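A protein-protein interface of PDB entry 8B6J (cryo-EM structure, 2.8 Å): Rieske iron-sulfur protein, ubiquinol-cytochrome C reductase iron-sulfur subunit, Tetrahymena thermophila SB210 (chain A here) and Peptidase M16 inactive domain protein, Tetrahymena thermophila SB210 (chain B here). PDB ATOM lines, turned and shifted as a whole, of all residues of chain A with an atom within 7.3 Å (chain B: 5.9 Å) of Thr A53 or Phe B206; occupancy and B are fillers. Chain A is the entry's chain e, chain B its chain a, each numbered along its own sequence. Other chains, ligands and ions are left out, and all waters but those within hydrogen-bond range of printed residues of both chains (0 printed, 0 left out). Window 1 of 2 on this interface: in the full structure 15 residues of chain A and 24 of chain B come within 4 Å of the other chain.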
ATOM      1  N   PHE A  51       1.741   4.787  11.993  1.00  0.00           N
ATOM      2  CA  PHE A  51       0.438   5.183  11.481  1.00  0.00           C
ATOM      3  C   PHE A  51      -0.588   5.095  12.599  1.00  0.00           C
ATOM      4  O   PHE A  51      -0.589   4.137  13.378  1.00  0.00           O
ATOM      5  CB  PHE A  51       0.004   4.293  10.315  1.00  0.00           C
ATOM      6  CG  PHE A  51       0.955   4.302   9.156  1.00  0.00           C
ATOM      7  CD1 PHE A  51       2.108   3.535   9.182  1.00  0.00           C
ATOM      8  CD2 PHE A  51       0.692   5.068   8.035  1.00  0.00           C
ATOM      9  CE1 PHE A  51       2.981   3.539   8.116  1.00  0.00           C
ATOM     10  CE2 PHE A  51       1.561   5.075   6.965  1.00  0.00           C
ATOM     11  CZ  PHE A  51       2.708   4.310   7.006  1.00  0.00           C
ATOM     12  N   VAL A  52      -1.460   6.095  12.673  1.00  0.00           N
ATOM     13  CA  VAL A  52      -2.528   6.129  13.661  1.00  0.00           C
ATOM     14  C   VAL A  52      -3.847   6.350  12.940  1.00  0.00           C
ATOM     15  O   VAL A  52      -3.894   6.945  11.858  1.00  0.00           O
ATOM     16  CB  VAL A  52      -2.298   7.226  14.723  1.00  0.00           C
ATOM     17  CG1 VAL A  52      -0.983   6.996  15.444  1.00  0.00           C
ATOM     18  CG2 VAL A  52      -2.328   8.604  14.083  1.00  0.00           C
ATOM     19  N   THR A  53      -4.925   5.861  13.545  1.00  0.00           N
ATOM     20  CA  THR A  53      -6.270   6.008  13.005  1.00  0.00           C
ATOM     21  C   THR A  53      -7.034   6.997  13.874  1.00  0.00           C
ATOM     22  O   THR A  53      -7.200   6.772  15.078  1.00  0.00           O
ATOM     23  CB  THR A  53      -6.997   4.665  12.958  1.00  0.00           C
ATOM     24  OG1 THR A  53      -7.147   4.152  14.285  1.00  0.00           O
ATOM     25  CG2 THR A  53      -6.223   3.666  12.117  1.00  0.00           C
ATOM     26  N   SER A  54      -7.498   8.085  13.262  1.00  0.00           N
ATOM     27  CA  SER A  54      -8.226   9.113  13.994  1.00  0.00           C
ATOM     28  C   SER A  54      -9.577   8.630  14.505  1.00  0.00           C
ATOM     29  O   SER A  54     -10.164   9.292  15.366  1.00  0.00           O
ATOM     30  CB  SER A  54      -8.421  10.338  13.103  1.00  0.00           C
ATOM     31  OG  SER A  54      -8.943   9.963  11.841  1.00  0.00           O
ATOM     32  N   SER A  55     -10.076   7.501  14.005  1.00  0.00           N
ATOM     33  CA  SER A  55     -11.354   6.947  14.429  1.00  0.00           C
ATOM     34  C   SER A  55     -11.190   5.877  15.501  1.00  0.00           C
ATOM     35  O   SER A  55     -12.116   5.093  15.734  1.00  0.00           O
ATOM     36  CB  SER A  55     -12.101   6.375  13.223  1.00  0.00           C
ATOM     37  OG  SER A  55     -13.381   5.901  13.597  1.00  0.00           O
ATOM     38  N   ARG A  56     -10.034   5.829  16.155  1.00  0.00           N
ATOM     39  CA  ARG A  56      -9.787   4.833  17.182  1.00  0.00           C
ATOM     40  C   ARG A  56     -10.625   5.130  18.421  1.00  0.00           C
ATOM     41  O   ARG A  56     -11.092   6.254  18.613  1.00  0.00           O
ATOM     42  CB  ARG A  56      -8.306   4.815  17.551  1.00  0.00           C
ATOM     43  CG  ARG A  56      -7.842   6.105  18.197  1.00  0.00           C
ATOM     44  CD  ARG A  56      -6.336   6.276  18.163  1.00  0.00           C
ATOM     45  NE  ARG A  56      -5.975   7.688  18.171  1.00  0.00           N
ATOM     46  CZ  ARG A  56      -4.751   8.152  18.381  1.00  0.00           C
ATOM     47  NH1 ARG A  56      -3.740   7.342  18.640  1.00  0.00           N
ATOM     48  NH2 ARG A  56      -4.538   9.464  18.335  1.00  0.00           N
ATOM     49  N   PRO A  57     -10.832   4.133  19.280  1.00  0.00           N
ATOM     50  CA  PRO A  57     -11.542   4.387  20.538  1.00  0.00           C
ATOM     51  C   PRO A  57     -10.828   5.428  21.384  1.00  0.00           C
ATOM     52  O   PRO A  57      -9.603   5.557  21.353  1.00  0.00           O
ATOM     53  CB  PRO A  57     -11.548   3.018  21.225  1.00  0.00           C
ATOM     54  CG  PRO A  57     -11.428   2.043  20.120  1.00  0.00           C
ATOM     55  CD  PRO A  57     -10.573   2.699  19.077  1.00  0.00           C
ATOM     56  N   PHE A  60      -7.876   4.562  23.694  1.00  0.00           N
ATOM     57  CA  PHE A  60      -6.548   4.399  23.121  1.00  0.00           C
ATOM     58  C   PHE A  60      -5.769   5.702  23.247  1.00  0.00           C
ATOM     59  O   PHE A  60      -6.321   6.791  23.068  1.00  0.00           O
ATOM     60  CB  PHE A  60      -6.634   3.993  21.648  1.00  0.00           C
ATOM     61  CG  PHE A  60      -7.149   2.597  21.418  1.00  0.00           C
ATOM     62  CD1 PHE A  60      -7.687   1.847  22.451  1.00  0.00           C
ATOM     63  CD2 PHE A  60      -7.084   2.032  20.157  1.00  0.00           C
ATOM     64  CE1 PHE A  60      -8.153   0.567  22.226  1.00  0.00           C
ATOM     65  CE2 PHE A  60      -7.548   0.752  19.928  1.00  0.00           C
ATOM     66  CZ  PHE A  60      -8.084   0.020  20.964  1.00  0.00           C
ATOM     67  N   HIS A  63       0.487   6.413  19.842  1.00  0.00           N
ATOM     68  CA  HIS A  63       1.117   5.209  19.324  1.00  0.00           C
ATOM     69  C   HIS A  63       2.361   4.870  20.135  1.00  0.00           C
ATOM     70  O   HIS A  63       3.178   5.741  20.445  1.00  0.00           O
ATOM     71  CB  HIS A  63       1.483   5.391  17.853  1.00  0.00           C
ATOM     72  CG  HIS A  63       1.851   4.116  17.160  1.00  0.00           C
ATOM     73  ND1 HIS A  63       2.953   3.367  17.515  1.00  0.00           N
ATOM     74  CD2 HIS A  63       1.266   3.458  16.133  1.00  0.00           C
ATOM     75  CE1 HIS A  63       3.028   2.302  16.738  1.00  0.00           C
ATOM     76  NE2 HIS A  63       2.017   2.335  15.889  1.00  0.00           N
ATOM     77  N   LEU B 201     -19.870   3.345  13.457  1.00  0.00           N
ATOM     78  CA  LEU B 201     -20.230   3.956  12.181  1.00  0.00           C
ATOM     79  C   LEU B 201     -19.094   4.832  11.661  1.00  0.00           C
ATOM     80  O   LEU B 201     -18.774   4.814  10.465  1.00  0.00           O
ATOM     81  CB  LEU B 201     -21.515   4.767  12.331  1.00  0.00           C
ATOM     82  CG  LEU B 201     -22.785   3.941  12.554  1.00  0.00           C
ATOM     83  CD1 LEU B 201     -23.956   4.848  12.887  1.00  0.00           C
ATOM     84  CD2 LEU B 201     -23.099   3.090  11.337  1.00  0.00           C
ATOM     85  N   GLU B 202     -18.463   5.596  12.551  1.00  0.00           N
ATOM     86  CA  GLU B 202     -17.306   6.386  12.143  1.00  0.00           C
ATOM     87  C   GLU B 202     -16.167   5.486  11.677  1.00  0.00           C
ATOM     88  O   GLU B 202     -15.447   5.821  10.731  1.00  0.00           O
ATOM     89  CB  GLU B 202     -16.853   7.286  13.290  1.00  0.00           C
ATOM     90  CG  GLU B 202     -17.872   8.353  13.662  1.00  0.00           C
ATOM     91  CD  GLU B 202     -17.364   9.307  14.724  1.00  0.00           C
ATOM     92  OE1 GLU B 202     -16.167   9.229  15.070  1.00  0.00           O
ATOM     93  OE2 GLU B 202     -18.161  10.135  15.212  1.00  0.00           O
ATOM     94  N   ASN B 203     -15.989   4.336  12.330  1.00  0.00           N
ATOM     95  CA  ASN B 203     -14.934   3.412  11.922  1.00  0.00           C
ATOM     96  C   ASN B 203     -15.205   2.819  10.544  1.00  0.00           C
ATOM     97  O   ASN B 203     -14.279   2.658   9.743  1.00  0.00           O
ATOM     98  CB  ASN B 203     -14.776   2.300  12.957  1.00  0.00           C
ATOM     99  CG  ASN B 203     -14.051   2.762  14.200  1.00  0.00           C
ATOM    100  OD1 ASN B 203     -12.832   2.922  14.198  1.00  0.00           O
ATOM    101  ND2 ASN B 203     -14.796   2.975  15.275  1.00  0.00           N
ATOM    102  N   ILE B 204     -16.459   2.463  10.253  1.00  0.00           N
ATOM    103  CA  ILE B 204     -16.764   1.942   8.922  1.00  0.00           C
ATOM    104  C   ILE B 204     -16.588   3.035   7.879  1.00  0.00           C
ATOM    105  O   ILE B 204     -16.179   2.764   6.746  1.00  0.00           O
ATOM    106  CB  ILE B 204     -18.176   1.330   8.855  1.00  0.00           C
ATOM    107  CG1 ILE B 204     -19.237   2.381   9.155  1.00  0.00           C
ATOM    108  CG2 ILE B 204     -18.297   0.161   9.810  1.00  0.00           C
ATOM    109  CD1 ILE B 204     -20.645   1.906   8.944  1.00  0.00           C
ATOM    110  N   HIS B 205     -16.909   4.282   8.227  1.00  0.00           N
ATOM    111  CA  HIS B 205     -16.632   5.374   7.299  1.00  0.00           C
ATOM    112  C   HIS B 205     -15.137   5.505   7.043  1.00  0.00           C
ATOM    113  O   HIS B 205     -14.707   5.693   5.900  1.00  0.00           O
ATOM    114  CB  HIS B 205     -17.203   6.684   7.834  1.00  0.00           C
ATOM    115  CG  HIS B 205     -18.677   6.828   7.622  1.00  0.00           C
ATOM    116  ND1 HIS B 205     -19.608   6.235   8.445  1.00  0.00           N
ATOM    117  CD2 HIS B 205     -19.380   7.490   6.674  1.00  0.00           C
ATOM    118  CE1 HIS B 205     -20.823   6.530   8.017  1.00  0.00           C
ATOM    119  NE2 HIS B 205     -20.711   7.290   6.943  1.00  0.00           N
ATOM    120  N   PHE B 206     -14.326   5.398   8.098  1.00  0.00           N
ATOM    121  CA  PHE B 206     -12.879   5.494   7.938  1.00  0.00           C
ATOM    122  C   PHE B 206     -12.341   4.369   7.062  1.00  0.00           C
ATOM    123  O   PHE B 206     -11.512   4.603   6.177  1.00  0.00           O
ATOM    124  CB  PHE B 206     -12.207   5.474   9.311  1.00  0.00           C
ATOM    125  CG  PHE B 206     -10.708   5.559   9.261  1.00  0.00           C
ATOM    126  CD1 PHE B 206      -9.940   4.417   9.118  1.00  0.00           C
ATOM    127  CD2 PHE B 206     -10.068   6.779   9.371  1.00  0.00           C
ATOM    128  CE1 PHE B 206      -8.564   4.493   9.075  1.00  0.00           C
ATOM    129  CE2 PHE B 206      -8.692   6.858   9.331  1.00  0.00           C
ATOM    130  CZ  PHE B 206      -7.940   5.714   9.183  1.00  0.00           C
ATOM    131  N   THR B 207     -12.800   3.139   7.296  1.00  0.00           N
ATOM    132  CA  THR B 207     -12.272   2.000   6.555  1.00  0.00           C
ATOM    133  C   THR B 207     -12.800   1.947   5.128  1.00  0.00           C
ATOM    134  O   THR B 207     -12.118   1.428   4.238  1.00  0.00           O
ATOM    135  CB  THR B 207     -12.603   0.694   7.282  1.00  0.00           C
ATOM    136  OG1 THR B 207     -11.765  -0.357   6.789  1.00  0.00           O
ATOM    137  CG2 THR B 207     -14.053   0.307   7.065  1.00  0.00           C
ATOM    138  N   ALA B 208     -14.004   2.468   4.887  1.00  0.00           N
ATOM    139  CA  ALA B 208     -14.584   2.425   3.552  1.00  0.00           C
ATOM    140  C   ALA B 208     -13.963   3.458   2.623  1.00  0.00           C
ATOM    141  O   ALA B 208     -13.820   3.196   1.424  1.00  0.00           O
ATOM    142  CB  ALA B 208     -16.095   2.641   3.631  1.00  0.00           C
ATOM    143  N   TYR B 209     -13.594   4.623   3.148  1.00  0.00           N
ATOM    144  CA  TYR B 209     -13.015   5.708   2.360  1.00  0.00           C
ATOM    145  C   TYR B 209     -11.661   6.061   2.967  1.00  0.00           C
ATOM    146  O   TYR B 209     -11.559   6.958   3.807  1.00  0.00           O
ATOM    147  CB  TYR B 209     -13.946   6.912   2.332  1.00  0.00           C
ATOM    148  CG  TYR B 209     -15.370   6.564   1.970  1.00  0.00           C
ATOM    149  CD1 TYR B 209     -15.723   6.285   0.660  1.00  0.00           C
ATOM    150  CD2 TYR B 209     -16.360   6.515   2.939  1.00  0.00           C
ATOM    151  CE1 TYR B 209     -17.020   5.966   0.325  1.00  0.00           C
ATOM    152  CE2 TYR B 209     -17.661   6.198   2.612  1.00  0.00           C
ATOM    153  CZ  TYR B 209     -17.985   5.925   1.303  1.00  0.00           C
ATOM    154  OH  TYR B 209     -19.280   5.608   0.968  1.00  0.00           O
ATOM    155  N   ARG B 210     -10.617   5.354   2.535  1.00  0.00           N
ATOM    156  CA  ARG B 210      -9.269   5.610   3.021  1.00  0.00           C
ATOM    157  C   ARG B 210      -8.517   6.626   2.175  1.00  0.00           C
ATOM    158  O   ARG B 210      -7.596   7.274   2.685  1.00  0.00           O
ATOM    159  CB  ARG B 210      -8.467   4.307   3.068  1.00  0.00           C
ATOM    160  CG  ARG B 210      -9.020   3.265   4.022  1.00  0.00           C
ATOM    161  CD  ARG B 210      -8.093   2.065   4.112  1.00  0.00           C
ATOM    162  NE  ARG B 210      -8.600   1.037   5.014  1.00  0.00           N
ATOM    163  CZ  ARG B 210      -8.468   1.063   6.333  1.00  0.00           C
ATOM    164  NH1 ARG B 210      -7.868   2.067   6.948  1.00  0.00           N
ATOM    165  NH2 ARG B 210      -8.955   0.056   7.053  1.00  0.00           N
ATOM    166  N   PHE B 214     -13.401  12.129   3.377  1.00  0.00           N
ATOM    167  CA  PHE B 214     -14.724  11.736   3.845  1.00  0.00           C
ATOM    168  C   PHE B 214     -14.655  10.624   4.882  1.00  0.00           C
ATOM    169  O   PHE B 214     -15.599  10.459   5.661  1.00  0.00           O
ATOM    170  CB  PHE B 214     -15.576  11.293   2.657  1.00  0.00           C
ATOM    171  CG  PHE B 214     -17.041  11.203   2.961  1.00  0.00           C
ATOM    172  CD1 PHE B 214     -17.594  10.024   3.428  1.00  0.00           C
ATOM    173  CD2 PHE B 214     -17.868  12.296   2.772  1.00  0.00           C
ATOM    174  CE1 PHE B 214     -18.941   9.939   3.705  1.00  0.00           C
ATOM    175  CE2 PHE B 214     -19.215  12.216   3.047  1.00  0.00           C
ATOM    176  CZ  PHE B 214     -19.753  11.036   3.514  1.00  0.00           C
ATOM    177  N   GLY B 215     -13.567   9.852   4.908  1.00  0.00           N
ATOM    178  CA  GLY B 215     -13.438   8.787   5.885  1.00  0.00           C
ATOM    179  C   GLY B 215     -13.074   9.248   7.278  1.00  0.00           C
ATOM    180  O   GLY B 215     -13.307   8.511   8.241  1.00  0.00           O
ATOM    181  N   GLN B 216     -12.516  10.448   7.413  1.00  0.00           N
ATOM    182  CA  GLN B 216     -12.057  10.906   8.711  1.00  0.00           C
ATOM    183  C   GLN B 216     -13.242  11.105   9.658  1.00  0.00           C
ATOM    184  O   GLN B 216     -14.346  11.440   9.223  1.00  0.00           O
ATOM    185  CB  GLN B 216     -11.275  12.208   8.571  1.00  0.00           C
ATOM    186  CG  GLN B 216     -10.071  12.105   7.646  1.00  0.00           C
ATOM    187  CD  GLN B 216      -9.077  11.051   8.093  1.00  0.00           C
ATOM    188  OE1 GLN B 216      -9.011  10.705   9.272  1.00  0.00           O
ATOM    189  NE2 GLN B 216      -8.300  10.532   7.150  1.00  0.00           N
ATOM    190  N   PRO B 217     -13.035  10.909  10.960  1.00  0.00           N
ATOM    191  CA  PRO B 217     -14.156  11.006  11.902  1.00  0.00           C
ATOM    192  C   PRO B 217     -14.734  12.413  11.953  1.00  0.00           C
ATOM    193  O   PRO B 217     -14.032  13.408  11.765  1.00  0.00           O
ATOM    194  CB  PRO B 217     -13.528  10.610  13.243  1.00  0.00           C
ATOM    195  CG  PRO B 217     -12.087  10.924  13.088  1.00  0.00           C
ATOM    196  CD  PRO B 217     -11.761  10.648  11.651  1.00  0.00           C
ATOM    197  N   ARG B 222      -7.915  14.246  17.113  1.00  0.00           N
ATOM    198  CA  ARG B 222      -7.767  14.787  18.460  1.00  0.00           C
ATOM    199  C   ARG B 222      -6.615  15.778  18.536  1.00  0.00           C
ATOM    200  O   ARG B 222      -6.781  16.910  19.003  1.00  0.00           O
ATOM    201  CB  ARG B 222      -7.541  13.653  19.460  1.00  0.00           C
ATOM    202  CG  ARG B 222      -8.541  12.525  19.379  1.00  0.00           C
ATOM    203  CD  ARG B 222      -8.122  11.389  20.285  1.00  0.00           C
ATOM    204  NE  ARG B 222      -8.862  10.168  20.003  1.00  0.00           N
ATOM    205  CZ  ARG B 222      -8.620   8.998  20.578  1.00  0.00           C
ATOM    206  NH1 ARG B 222      -7.663   8.856  21.480  1.00  0.00           N
ATOM    207  NH2 ARG B 222      -9.355   7.945  20.236  1.00  0.00           N
ATOM    208  N   MET B 292     -11.157  -3.941   9.192  1.00  0.00           N
ATOM    209  CA  MET B 292     -10.440  -3.393  10.336  1.00  0.00           C
ATOM    210  C   MET B 292     -10.835  -4.133  11.609  1.00  0.00           C
ATOM    211  O   MET B 292     -11.991  -4.537  11.775  1.00  0.00           O
ATOM    212  CB  MET B 292     -10.731  -1.899  10.494  1.00  0.00           C
ATOM    213  CG  MET B 292      -9.853  -1.200  11.523  1.00  0.00           C
ATOM    214  SD  MET B 292     -10.467   0.428  11.992  1.00  0.00           S
ATOM    215  CE  MET B 292     -10.374   1.298  10.434  1.00  0.00           C
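Among the printed residues, pairs that only touch across the chains: Ser A54 with Pro B217, Ser A55 with Glu B202 and Thr A53 with Phe B206.
The backbone NH of Phe B206 sits close to the backbone carbonyl oxygen of Gly B215 (3.3 Å).
The backbone carbonyl oxygen of Thr A53 lies close to the guanidinium group of Arg A56 (3.5 Å).
Hydrophobic or aromatic side chains of chain B that line the printed part of chain A: Phe B206 and Pro B217.
Printed residues of chain A that touch a printed residue of chain B: Thr A53, Ser A54, Ser A55, Arg A56, Pro A57 and Phe A60.
Among the printed residues, 8 pairs touch across the chains.
Of the printed residues of chain B, Thr A53 touches Phe B206.
Printed residues of chain B within 4 Å of Ser A54: Gln B216 and Pro B217.
Of the printed residues of chain A, Glu B202 touches Ser A55 (3.4 Å).
Of the printed residues of chain A, Phe B206 touches Thr A53 (3.9 Å).
Gly B215 touches none of the printed residues of chain A.
The nearest residue of chain B that does not touch Thr A53 is Met B292 (5.1 Å).
The guanidinium group (NH2) of Arg B222 lies within hydrogen-bond range of the backbone carbonyl oxygen (O) of Arg A56, at 2.9 Å.
The backbone carbonyl oxygen (O) of Ser A55 lies close to the side-chain amide oxygen (OD1) of Asn B203, 2.8 Å away.
NH1 of Arg B222 lies within hydrogen-bond range of O of Phe A60 (2.9 Å).
The backbone carbonyl oxygen (O) of Pro A57 is in hydrogen-bond range of the guanidinium group (NH2) of Arg B222, at 2.6 Å.
The side-chain amide oxygen (OE1) of Gln B216 is in hydrogen-bond range of the side-chain hydroxyl (OG) of Ser A54 (2.7 Å).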
